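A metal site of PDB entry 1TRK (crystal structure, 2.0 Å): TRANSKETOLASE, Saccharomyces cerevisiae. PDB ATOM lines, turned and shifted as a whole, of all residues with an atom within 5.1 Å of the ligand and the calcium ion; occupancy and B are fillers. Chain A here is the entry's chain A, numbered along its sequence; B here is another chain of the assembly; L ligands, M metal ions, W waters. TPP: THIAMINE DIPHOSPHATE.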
ATOM      1  N   ALA A  33      18.261  24.951  -5.323  1.00  0.00           N
ATOM      2  CA  ALA A  33      18.322  23.642  -4.694  1.00  0.00           C
ATOM      3  C   ALA A  33      19.553  23.456  -3.790  1.00  0.00           C
ATOM      4  O   ALA A  33      19.372  22.799  -2.748  1.00  0.00           O
ATOM      5  CB  ALA A  33      18.331  22.539  -5.758  1.00  0.00           C
ATOM      6  N   ASN A  67      20.408  15.741  -9.738  1.00  0.00           N
ATOM      7  CA  ASN A  67      20.004  17.088 -10.111  1.00  0.00           C
ATOM      8  C   ASN A  67      21.253  17.946 -10.253  1.00  0.00           C
ATOM      9  O   ASN A  67      21.454  18.913  -9.535  1.00  0.00           O
ATOM     10  CB  ASN A  67      19.055  17.675  -9.054  1.00  0.00           C
ATOM     11  CG  ASN A  67      19.360  17.371  -7.594  1.00  0.00           C
ATOM     12  OD1 ASN A  67      18.744  17.952  -6.712  1.00  0.00           O
ATOM     13  ND2 ASN A  67      20.241  16.524  -7.163  1.00  0.00           N
ATOM     14  N   HIS A  69      22.366  20.536 -11.687  1.00  0.00           N
ATOM     15  CA  HIS A  69      22.452  21.978 -11.673  1.00  0.00           C
ATOM     16  C   HIS A  69      22.628  22.539 -10.288  1.00  0.00           C
ATOM     17  O   HIS A  69      22.888  23.725 -10.198  1.00  0.00           O
ATOM     18  CB  HIS A  69      21.220  22.667 -12.268  1.00  0.00           C
ATOM     19  CG  HIS A  69      19.969  22.202 -11.606  1.00  0.00           C
ATOM     20  ND1 HIS A  69      19.276  21.127 -11.939  1.00  0.00           N
ATOM     21  CD2 HIS A  69      19.395  22.752 -10.471  1.00  0.00           C
ATOM     22  CE1 HIS A  69      18.327  20.957 -11.066  1.00  0.00           C
ATOM     23  NE2 HIS A  69      18.419  21.934 -10.191  1.00  0.00           N
ATOM     24  N   GLY A 116      23.803  16.567 -14.968  1.00  0.00           N
ATOM     25  CA  GLY A 116      23.369  17.838 -15.570  1.00  0.00           C
ATOM     26  C   GLY A 116      22.151  17.618 -16.491  1.00  0.00           C
ATOM     27  O   GLY A 116      21.030  18.083 -16.192  1.00  0.00           O
ATOM     28  N   PRO A 117      22.290  16.872 -17.620  1.00  0.00           N
ATOM     29  CA  PRO A 117      21.176  16.224 -18.318  1.00  0.00           C
ATOM     30  C   PRO A 117      20.327  15.407 -17.330  1.00  0.00           C
ATOM     31  O   PRO A 117      20.770  14.410 -16.728  1.00  0.00           O
ATOM     32  CB  PRO A 117      21.834  15.344 -19.379  1.00  0.00           C
ATOM     33  CG  PRO A 117      23.121  16.079 -19.605  1.00  0.00           C
ATOM     34  CD  PRO A 117      23.534  16.363 -18.166  1.00  0.00           C
ATOM     35  N   LEU A 118      19.086  15.823 -17.128  1.00  0.00           N
ATOM     36  CA  LEU A 118      18.213  15.179 -16.129  1.00  0.00           C
ATOM     37  C   LEU A 118      17.852  13.720 -16.392  1.00  0.00           C
ATOM     38  O   LEU A 118      17.694  13.279 -17.524  1.00  0.00           O
ATOM     39  CB  LEU A 118      16.938  15.991 -15.980  1.00  0.00           C
ATOM     40  CG  LEU A 118      17.111  17.433 -15.585  1.00  0.00           C
ATOM     41  CD1 LEU A 118      15.817  18.212 -15.781  1.00  0.00           C
ATOM     42  CD2 LEU A 118      17.573  17.469 -14.126  1.00  0.00           C
ATOM     43  N   GLY A 156      15.753  15.593  -8.078  1.00  0.00           N
ATOM     44  CA  GLY A 156      14.709  16.601  -8.019  1.00  0.00           C
ATOM     45  C   GLY A 156      13.512  16.247  -8.892  1.00  0.00           C
ATOM     46  O   GLY A 156      13.366  15.121  -9.410  1.00  0.00           O
ATOM     47  N   ASP A 157      12.587  17.175  -9.053  1.00  0.00           N
ATOM     48  CA  ASP A 157      11.404  16.936  -9.902  1.00  0.00           C
ATOM     49  C   ASP A 157      11.635  16.639 -11.366  1.00  0.00           C
ATOM     50  O   ASP A 157      11.041  15.722 -11.939  1.00  0.00           O
ATOM     51  CB  ASP A 157      10.456  18.109  -9.847  1.00  0.00           C
ATOM     52  CG  ASP A 157       9.888  18.356  -8.443  1.00  0.00           C
ATOM     53  OD1 ASP A 157       9.051  17.544  -8.017  1.00  0.00           O
ATOM     54  OD2 ASP A 157      10.290  19.331  -7.778  1.00  0.00           O
ATOM     55  N   GLY A 158      12.504  17.416 -12.026  1.00  0.00           N
ATOM     56  CA  GLY A 158      12.904  17.135 -13.412  1.00  0.00           C
ATOM     57  C   GLY A 158      13.378  15.710 -13.700  1.00  0.00           C
ATOM     58  O   GLY A 158      12.980  15.071 -14.683  1.00  0.00           O
ATOM     59  N   CYS A 159      14.225  15.195 -12.809  1.00  0.00           N
ATOM     60  CA  CYS A 159      14.693  13.800 -12.893  1.00  0.00           C
ATOM     61  C   CYS A 159      13.537  12.796 -12.865  1.00  0.00           C
ATOM     62  O   CYS A 159      13.548  11.812 -13.609  1.00  0.00           O
ATOM     63  CB  CYS A 159      15.628  13.419 -11.742  1.00  0.00           C
ATOM     64  SG  CYS A 159      17.313  14.141 -11.874  1.00  0.00           S
ATOM     65  N   GLU A 162      11.543  12.739 -16.393  1.00  0.00           N
ATOM     66  CA  GLU A 162      12.237  12.089 -17.478  1.00  0.00           C
ATOM     67  C   GLU A 162      11.995  10.578 -17.512  1.00  0.00           C
ATOM     68  O   GLU A 162      12.166   9.887 -16.506  1.00  0.00           O
ATOM     69  CB  GLU A 162      13.703  12.327 -17.354  1.00  0.00           C
ATOM     70  CG  GLU A 162      14.131  13.723 -17.783  1.00  0.00           C
ATOM     71  CD  GLU A 162      14.034  13.992 -19.310  1.00  0.00           C
ATOM     72  OE1 GLU A 162      13.698  13.111 -20.102  1.00  0.00           O
ATOM     73  OE2 GLU A 162      14.342  15.116 -19.701  1.00  0.00           O
ATOM     74  N   ASP A 185      14.277  15.714  -3.471  1.00  0.00           N
ATOM     75  CA  ASP A 185      14.061  17.094  -3.074  1.00  0.00           C
ATOM     76  C   ASP A 185      12.657  17.573  -3.487  1.00  0.00           C
ATOM     77  O   ASP A 185      12.391  18.161  -4.548  1.00  0.00           O
ATOM     78  CB  ASP A 185      15.165  17.955  -3.700  1.00  0.00           C
ATOM     79  CG  ASP A 185      15.044  19.483  -3.412  1.00  0.00           C
ATOM     80  OD1 ASP A 185      14.433  19.868  -2.421  1.00  0.00           O
ATOM     81  OD2 ASP A 185      15.564  20.295  -4.166  1.00  0.00           O
ATOM     82  N   ASN A 187      10.376  20.015  -3.722  1.00  0.00           N
ATOM     83  CA  ASN A 187      10.187  21.421  -3.424  1.00  0.00           C
ATOM     84  C   ASN A 187       9.072  22.133  -4.161  1.00  0.00           C
ATOM     85  O   ASN A 187       8.957  23.350  -4.054  1.00  0.00           O
ATOM     86  CB  ASN A 187      11.524  22.210  -3.641  1.00  0.00           C
ATOM     87  CG  ASN A 187      12.103  22.147  -5.031  1.00  0.00           C
ATOM     88  OD1 ASN A 187      11.441  21.738  -5.979  1.00  0.00           O
ATOM     89  ND2 ASN A 187      13.364  22.499  -5.246  1.00  0.00           N
ATOM     90  N   LYS A 188       8.228  21.468  -4.955  1.00  0.00           N
ATOM     91  CA  LYS A 188       7.057  22.058  -5.618  1.00  0.00           C
ATOM     92  C   LYS A 188       7.203  23.042  -6.758  1.00  0.00           C
ATOM     93  O   LYS A 188       6.200  23.502  -7.313  1.00  0.00           O
ATOM     94  CB  LYS A 188       6.124  22.741  -4.599  1.00  0.00           C
ATOM     95  CG  LYS A 188       5.075  21.816  -4.009  1.00  0.00           C
ATOM     96  CD  LYS A 188       5.654  20.831  -3.025  1.00  0.00           C
ATOM     97  CE  LYS A 188       4.562  19.899  -2.539  1.00  0.00           C
ATOM     98  NZ  LYS A 188       5.102  18.826  -1.724  1.00  0.00           N
ATOM     99  N   ILE A 189       8.445  23.285  -7.148  1.00  0.00           N
ATOM    100  CA  ILE A 189       8.826  24.232  -8.185  1.00  0.00           C
ATOM    101  C   ILE A 189       9.726  23.599  -9.267  1.00  0.00           C
ATOM    102  O   ILE A 189      10.649  22.840  -8.997  1.00  0.00           O
ATOM    103  CB  ILE A 189       9.553  25.408  -7.397  1.00  0.00           C
ATOM    104  CG1 ILE A 189       8.489  26.443  -6.961  1.00  0.00           C
ATOM    105  CG2 ILE A 189      10.741  25.990  -8.209  1.00  0.00           C
ATOM    106  CD1 ILE A 189       7.860  27.350  -8.044  1.00  0.00           C
ATOM    107  N   THR A 190       9.500  23.874 -10.534  1.00  0.00           N
ATOM    108  CA  THR A 190      10.482  23.544 -11.569  1.00  0.00           C
ATOM    109  C   THR A 190      10.738  24.801 -12.408  1.00  0.00           C
ATOM    110  O   THR A 190      10.302  25.893 -11.993  1.00  0.00           O
ATOM    111  CB  THR A 190      10.017  22.400 -12.533  1.00  0.00           C
ATOM    112  OG1 THR A 190       8.881  22.894 -13.234  1.00  0.00           O
ATOM    113  CG2 THR A 190       9.695  21.082 -11.823  1.00  0.00           C
ATOM    114  N   ILE A 191      11.391  24.816 -13.573  1.00  0.00           N
ATOM    115  CA  ILE A 191      11.594  26.101 -14.276  1.00  0.00           C
ATOM    116  C   ILE A 191      10.294  26.843 -14.644  1.00  0.00           C
ATOM    117  O   ILE A 191      10.228  28.064 -14.456  1.00  0.00           O
ATOM    118  CB  ILE A 191      12.450  25.864 -15.538  1.00  0.00           C
ATOM    119  CG1 ILE A 191      13.847  25.543 -15.084  1.00  0.00           C
ATOM    120  CG2 ILE A 191      12.435  27.041 -16.509  1.00  0.00           C
ATOM    121  CD1 ILE A 191      14.833  25.332 -16.210  1.00  0.00           C
ATOM    122  N   ILE A 250      12.488  25.592  -1.979  1.00  0.00           N
ATOM    123  CA  ILE A 250      13.536  26.064  -2.885  1.00  0.00           C
ATOM    124  C   ILE A 250      14.112  27.416  -2.436  1.00  0.00           C
ATOM    125  O   ILE A 250      13.370  28.300  -1.993  1.00  0.00           O
ATOM    126  CB  ILE A 250      12.971  26.145  -4.355  1.00  0.00           C
ATOM    127  CG1 ILE A 250      14.196  26.238  -5.259  1.00  0.00           C
ATOM    128  CG2 ILE A 250      11.947  27.265  -4.559  1.00  0.00           C
ATOM    129  CD1 ILE A 250      14.025  25.784  -6.732  1.00  0.00           C
ATOM    130  N   HIS A 263      15.462  29.609  -8.957  1.00  0.00           N
ATOM    131  CA  HIS A 263      16.025  28.369  -9.510  1.00  0.00           C
ATOM    132  C   HIS A 263      17.392  28.494 -10.229  1.00  0.00           C
ATOM    133  O   HIS A 263      18.312  27.697 -10.010  1.00  0.00           O
ATOM    134  CB  HIS A 263      14.989  27.730 -10.488  1.00  0.00           C
ATOM    135  CG  HIS A 263      15.558  26.669 -11.457  1.00  0.00           C
ATOM    136  ND1 HIS A 263      15.748  25.383 -11.171  1.00  0.00           N
ATOM    137  CD2 HIS A 263      16.034  26.904 -12.735  1.00  0.00           C
ATOM    138  CE1 HIS A 263      16.330  24.828 -12.205  1.00  0.00           C
ATOM    139  NE2 HIS A 263      16.495  25.746 -13.121  1.00  0.00           N
ATOM    140  N   ALA B 381       9.126  22.176 -23.073  1.00  0.00           N
ATOM    141  CA  ALA B 381       9.400  21.126 -22.120  1.00  0.00           C
ATOM    142  C   ALA B 381      10.065  21.699 -20.831  1.00  0.00           C
ATOM    143  O   ALA B 381      11.253  21.519 -20.470  1.00  0.00           O
ATOM    144  CB  ALA B 381      10.280  20.074 -22.834  1.00  0.00           C
ATOM    145  N   ASP B 382       9.240  22.491 -20.117  1.00  0.00           N
ATOM    146  CA  ASP B 382       9.644  23.262 -18.932  1.00  0.00           C
ATOM    147  C   ASP B 382      10.718  24.312 -19.170  1.00  0.00           C
ATOM    148  O   ASP B 382      11.454  24.703 -18.289  1.00  0.00           O
ATOM    149  CB  ASP B 382      10.104  22.290 -17.840  1.00  0.00           C
ATOM    150  CG  ASP B 382      10.174  22.890 -16.446  1.00  0.00           C
ATOM    151  OD1 ASP B 382       9.120  23.277 -15.946  1.00  0.00           O
ATOM    152  OD2 ASP B 382      11.287  22.958 -15.902  1.00  0.00           O
ATOM    153  N   LEU B 383      10.834  24.884 -20.351  1.00  0.00           N
ATOM    154  CA  LEU B 383      11.836  25.909 -20.608  1.00  0.00           C
ATOM    155  C   LEU B 383      11.237  27.151 -21.229  1.00  0.00           C
ATOM    156  O   LEU B 383      11.927  27.919 -21.910  1.00  0.00           O
ATOM    157  CB  LEU B 383      12.916  25.367 -21.531  1.00  0.00           C
ATOM    158  CG  LEU B 383      14.006  24.584 -20.860  1.00  0.00           C
ATOM    159  CD1 LEU B 383      14.819  23.802 -21.906  1.00  0.00           C
ATOM    160  CD2 LEU B 383      14.815  25.574 -19.978  1.00  0.00           C
ATOM    161  N   ILE B 416       9.262  18.173 -18.041  1.00  0.00           N
ATOM    162  CA  ILE B 416      10.580  17.819 -18.516  1.00  0.00           C
ATOM    163  C   ILE B 416      10.474  16.427 -19.124  1.00  0.00           C
ATOM    164  O   ILE B 416      10.917  15.394 -18.624  1.00  0.00           O
ATOM    165  CB  ILE B 416      11.599  17.844 -17.370  1.00  0.00           C
ATOM    166  CG1 ILE B 416      11.710  19.227 -16.689  1.00  0.00           C
ATOM    167  CG2 ILE B 416      12.978  17.712 -17.992  1.00  0.00           C
ATOM    168  CD1 ILE B 416      10.798  19.409 -15.443  1.00  0.00           C
ATOM    169  N   GLU B 418      10.907  15.592 -23.017  1.00  0.00           N
ATOM    170  CA  GLU B 418      11.166  15.837 -24.445  1.00  0.00           C
ATOM    171  C   GLU B 418      10.759  14.696 -25.400  1.00  0.00           C
ATOM    172  O   GLU B 418      10.201  14.962 -26.461  1.00  0.00           O
ATOM    173  CB  GLU B 418      12.607  16.102 -24.732  1.00  0.00           C
ATOM    174  CG  GLU B 418      13.196  17.231 -23.897  1.00  0.00           C
ATOM    175  CD  GLU B 418      13.656  16.877 -22.471  1.00  0.00           C
ATOM    176  OE1 GLU B 418      13.649  15.692 -22.142  1.00  0.00           O
ATOM    177  OE2 GLU B 418      14.045  17.772 -21.728  1.00  0.00           O
ATOM    178  N   PHE B 442      16.057  22.960 -25.220  1.00  0.00           N
ATOM    179  CA  PHE B 442      17.405  23.276 -25.687  1.00  0.00           C
ATOM    180  C   PHE B 442      17.762  22.288 -26.794  1.00  0.00           C
ATOM    181  O   PHE B 442      17.412  21.085 -26.775  1.00  0.00           O
ATOM    182  CB  PHE B 442      18.454  23.117 -24.558  1.00  0.00           C
ATOM    183  CG  PHE B 442      18.256  24.097 -23.403  1.00  0.00           C
ATOM    184  CD1 PHE B 442      17.669  25.342 -23.617  1.00  0.00           C
ATOM    185  CD2 PHE B 442      18.731  23.799 -22.144  1.00  0.00           C
ATOM    186  CE1 PHE B 442      17.604  26.268 -22.579  1.00  0.00           C
ATOM    187  CE2 PHE B 442      18.652  24.735 -21.107  1.00  0.00           C
ATOM    188  CZ  PHE B 442      18.100  25.971 -21.314  1.00  0.00           C
ATOM    189  N   PHE B 445      19.072  18.671 -26.030  1.00  0.00           N
ATOM    190  CA  PHE B 445      18.183  17.670 -25.506  1.00  0.00           C
ATOM    191  C   PHE B 445      17.036  17.326 -26.456  1.00  0.00           C
ATOM    192  O   PHE B 445      16.261  16.413 -26.177  1.00  0.00           O
ATOM    193  CB  PHE B 445      17.629  18.136 -24.130  1.00  0.00           C
ATOM    194  CG  PHE B 445      18.759  18.478 -23.128  1.00  0.00           C
ATOM    195  CD1 PHE B 445      19.787  17.582 -22.908  1.00  0.00           C
ATOM    196  CD2 PHE B 445      18.743  19.699 -22.484  1.00  0.00           C
ATOM    197  CE1 PHE B 445      20.827  17.909 -22.048  1.00  0.00           C
ATOM    198  CE2 PHE B 445      19.776  20.015 -21.628  1.00  0.00           C
ATOM    199  CZ  PHE B 445      20.818  19.130 -21.412  1.00  0.00           C
ATOM    200  N   TYR B 448      17.160  13.727 -26.789  1.00  0.00           N
ATOM    201  CA  TYR B 448      16.404  12.837 -25.897  1.00  0.00           C
ATOM    202  C   TYR B 448      15.159  12.273 -26.612  1.00  0.00           C
ATOM    203  O   TYR B 448      14.634  11.217 -26.258  1.00  0.00           O
ATOM    204  CB  TYR B 448      15.962  13.601 -24.648  1.00  0.00           C
ATOM    205  CG  TYR B 448      16.850  13.465 -23.409  1.00  0.00           C
ATOM    206  CD1 TYR B 448      18.226  13.654 -23.450  1.00  0.00           C
ATOM    207  CD2 TYR B 448      16.248  13.132 -22.214  1.00  0.00           C
ATOM    208  CE1 TYR B 448      19.001  13.512 -22.295  1.00  0.00           C
ATOM    209  CE2 TYR B 448      16.994  12.977 -21.070  1.00  0.00           C
ATOM    210  CZ  TYR B 448      18.363  13.175 -21.118  1.00  0.00           C
ATOM    211  OH  TYR B 448      19.067  13.051 -19.961  1.00  0.00           O
ATOM    212  N   HIS B 481      25.732  20.788 -21.920  1.00  0.00           N
ATOM    213  CA  HIS B 481      24.601  21.555 -22.491  1.00  0.00           C
ATOM    214  C   HIS B 481      24.877  22.204 -23.862  1.00  0.00           C
ATOM    215  O   HIS B 481      24.000  22.800 -24.484  1.00  0.00           O
ATOM    216  CB  HIS B 481      24.178  22.680 -21.536  1.00  0.00           C
ATOM    217  CG  HIS B 481      23.434  22.156 -20.308  1.00  0.00           C
ATOM    218  ND1 HIS B 481      23.808  21.245 -19.391  1.00  0.00           N
ATOM    219  CD2 HIS B 481      22.147  22.549 -19.984  1.00  0.00           C
ATOM    220  CE1 HIS B 481      22.827  21.046 -18.568  1.00  0.00           C
ATOM    221  NE2 HIS B 481      21.853  21.839 -18.940  1.00  0.00           N
HETATM  222  N1' TPP L   1      16.333  18.608 -20.115  1.00  0.00           N
HETATM  223  C2' TPP L   1      17.317  17.803 -19.627  1.00  0.00           C
HETATM  224  CM2 TPP L   1      17.320  16.405 -20.034  1.00  0.00           C
HETATM  225  N3' TPP L   1      18.283  18.243 -18.871  1.00  0.00           N
HETATM  226  C4' TPP L   1      18.226  19.539 -18.459  1.00  0.00           C
HETATM  227  N4' TPP L   1      19.178  19.919 -17.628  1.00  0.00           N
HETATM  228  C5' TPP L   1      17.199  20.437 -18.929  1.00  0.00           C
HETATM  229  C6' TPP L   1      16.278  19.914 -19.769  1.00  0.00           C
HETATM  230  C7' TPP L   1      17.094  21.870 -18.470  1.00  0.00           C
HETATM  231  N3  TPP L   1      16.757  21.855 -16.978  1.00  0.00           N
HETATM  232  C2  TPP L   1      17.655  22.004 -15.993  1.00  0.00           C
HETATM  233  S1  TPP L   1      16.966  22.043 -14.468  1.00  0.00           S
HETATM  234  C5  TPP L   1      15.393  21.871 -15.198  1.00  0.00           C
HETATM  235  C4  TPP L   1      15.494  21.799 -16.550  1.00  0.00           C
HETATM  236  CM4 TPP L   1      14.340  21.797 -17.510  1.00  0.00           C
HETATM  237  C6  TPP L   1      14.111  21.989 -14.423  1.00  0.00           C
HETATM  238  C7  TPP L   1      14.141  22.126 -12.939  1.00  0.00           C
HETATM  239  O7  TPP L   1      14.215  20.769 -12.426  1.00  0.00           O
HETATM  240  PA  TPP L   1      14.116  20.518 -10.872  1.00  0.00           P
HETATM  241  O1A TPP L   1      14.812  19.216 -10.730  1.00  0.00           O
HETATM  242  O2A TPP L   1      12.697  20.614 -10.478  1.00  0.00           O
HETATM  243  O3A TPP L   1      14.896  21.758 -10.205  1.00  0.00           O
HETATM  244  PB  TPP L   1      15.167  22.361  -8.770  1.00  0.00           P
HETATM  245  O1B TPP L   1      13.892  22.184  -8.072  1.00  0.00           O
HETATM  246  O2B TPP L   1      15.579  23.764  -8.947  1.00  0.00           O
HETATM  247  O3B TPP L   1      16.237  21.445  -8.299  1.00  0.00           O
HETATM  248 CA    CA M   1      11.949  21.028  -8.082  1.00  0.00          CA
HETATM  249  O   HOH W   1      18.192  25.200  -8.644  1.00  0.00           O
HETATM  250  O   HOH W   2      13.588  20.672 -21.663  1.00  0.00           O
HETATM  251  O   HOH W   3      16.187  19.527  -6.799  1.00  0.00           O
HETATM  252  O   HOH W   4      13.161  19.438  -7.151  1.00  0.00           O
HETATM  253  O   HOH W   5      16.127  16.714 -11.151  1.00  0.00           O
HETATM  254  O   HOH W   6      20.869  22.433 -15.973  1.00  0.00           O
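An oxygen (O1A) of the ligand sits at hydrogen-bond distance from the backbone NH of Asp 157.
A ring nitrogen (ND1) of His 263 lies within hydrogen-bond range of an oxygen (O2B) of the ligand, 2.8 Å away.
An oxygen (O3B) of the ligand sits at hydrogen-bond distance from a ring nitrogen (NE2) of His 69, at 2.9 Å.
A nitrogen (N4') of the ligand lies within hydrogen-bond range of the backbone carbonyl oxygen (O) of Gly 116, 3.0 Å away.
N of Leu 118 lies within hydrogen-bond range of N3' of the ligand (3.1 Å).
The backbone NH of Gly 158 is in hydrogen-bond range of an oxygen (O1A) of the ligand (3.2 Å).
The side-chain amide nitrogen of Asn 187 lies within hydrogen-bond range of the side-chain carboxylate of Asp 185 (3.3 Å).
The side-chain carboxylate (OE1) of Glu 418 of chain B lies close to the side-chain carboxylate (OE2) of Glu 162.
The backbone carbonyl oxygen (O) of Leu 118 sits at hydrogen-bond distance from the side-chain hydroxyl (OH) of Tyr 448 of chain B, at 2.8 Å.
The side-chain hydroxyl (OG1) of Thr 190 lies within hydrogen-bond range of the side-chain carboxylate (OD1) of Asp 382 of chain B.
OD2 of Asp 382 of chain B lies within hydrogen-bond range of N of Ile 191, at 3.0 Å.
The side-chain carboxylate of Glu 418 of chain B lies close to a nitrogen (N1') of the ligand (2.9 Å).
Merely in contact with the ligand: Ala 33 (3.5 Å), Pro 117 (3.6 Å), Gly 156 (3.7 Å), Glu 162 (3.3 Å), Thr 190 (3.3 Å), Ile 191 (3.6 Å), Ile 250 (3.4 Å), Asp 382 of chain B (3.3 Å), Ile 416 of chain B (3.8 Å), Phe 445 of chain B (3.6 Å), Tyr 448 of chain B (3.6 Å) and His 481 of chain B (3.5 Å).
Within 4 Å of the ligand: Ala 33, His 69, Gly 116, Pro 117, Leu 118, Gly 156, Asp 157, Gly 158, Glu 162, Asn 187, Ile 189, Thr 190, Ile 191, Ile 250, His 263, Asp 382 of chain B, Ile 416 of chain B, Glu 418 of chain B, Phe 445 of chain B, Tyr 448 of chain B and His 481 of chain B.
Along chain A the residues within 4 Å of the ligand span positions 33 to 263.
The nearest printed residue that does not touch the ligand is Phe 442 of chain B (4.2 Å).
Of the 28 residues printed, 3 come within 4 Å of the calcium ion.
The nearest printed residue that does not touch the calcium ion is Thr 190 (4.4 Å).
The calcium ion is bound by water W4 (2.2 Å), O1B of the ligand (2.3 Å), OD1 of Asn 187 (2.3 Å), OD2 of Asp 157 (2.4 Å), O of Ile 189 (2.4 Å) and O2A of the ligand (2.5 Å).
Water W4 bridges O of Asp 185 and N of Asp 157.
Water W3 lies within hydrogen-bond range of O3B of the ligand (2.4 Å), OD2 of Asp 185 (2.8 Å) and OD1 of Asn 67 (3.0 Å).
Water W5 lies within hydrogen-bond range of O1A of the ligand (2.9 Å), SG of Cys 159 (2.9 Å) and N of Gly 156 (3.3 Å).
Water W1 lies within hydrogen-bond range of O of His 263, O2B of the ligand and N of Ala 33.
Water W6 bridges NE2 of His 481 of chain B (3.2 Å) and N4' of the ligand (3.5 Å).
Water W2 lies within hydrogen-bond range of O of Ala 381 of chain B (2.8 Å) and OE2 of Glu 418 of chain B (2.9 Å).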
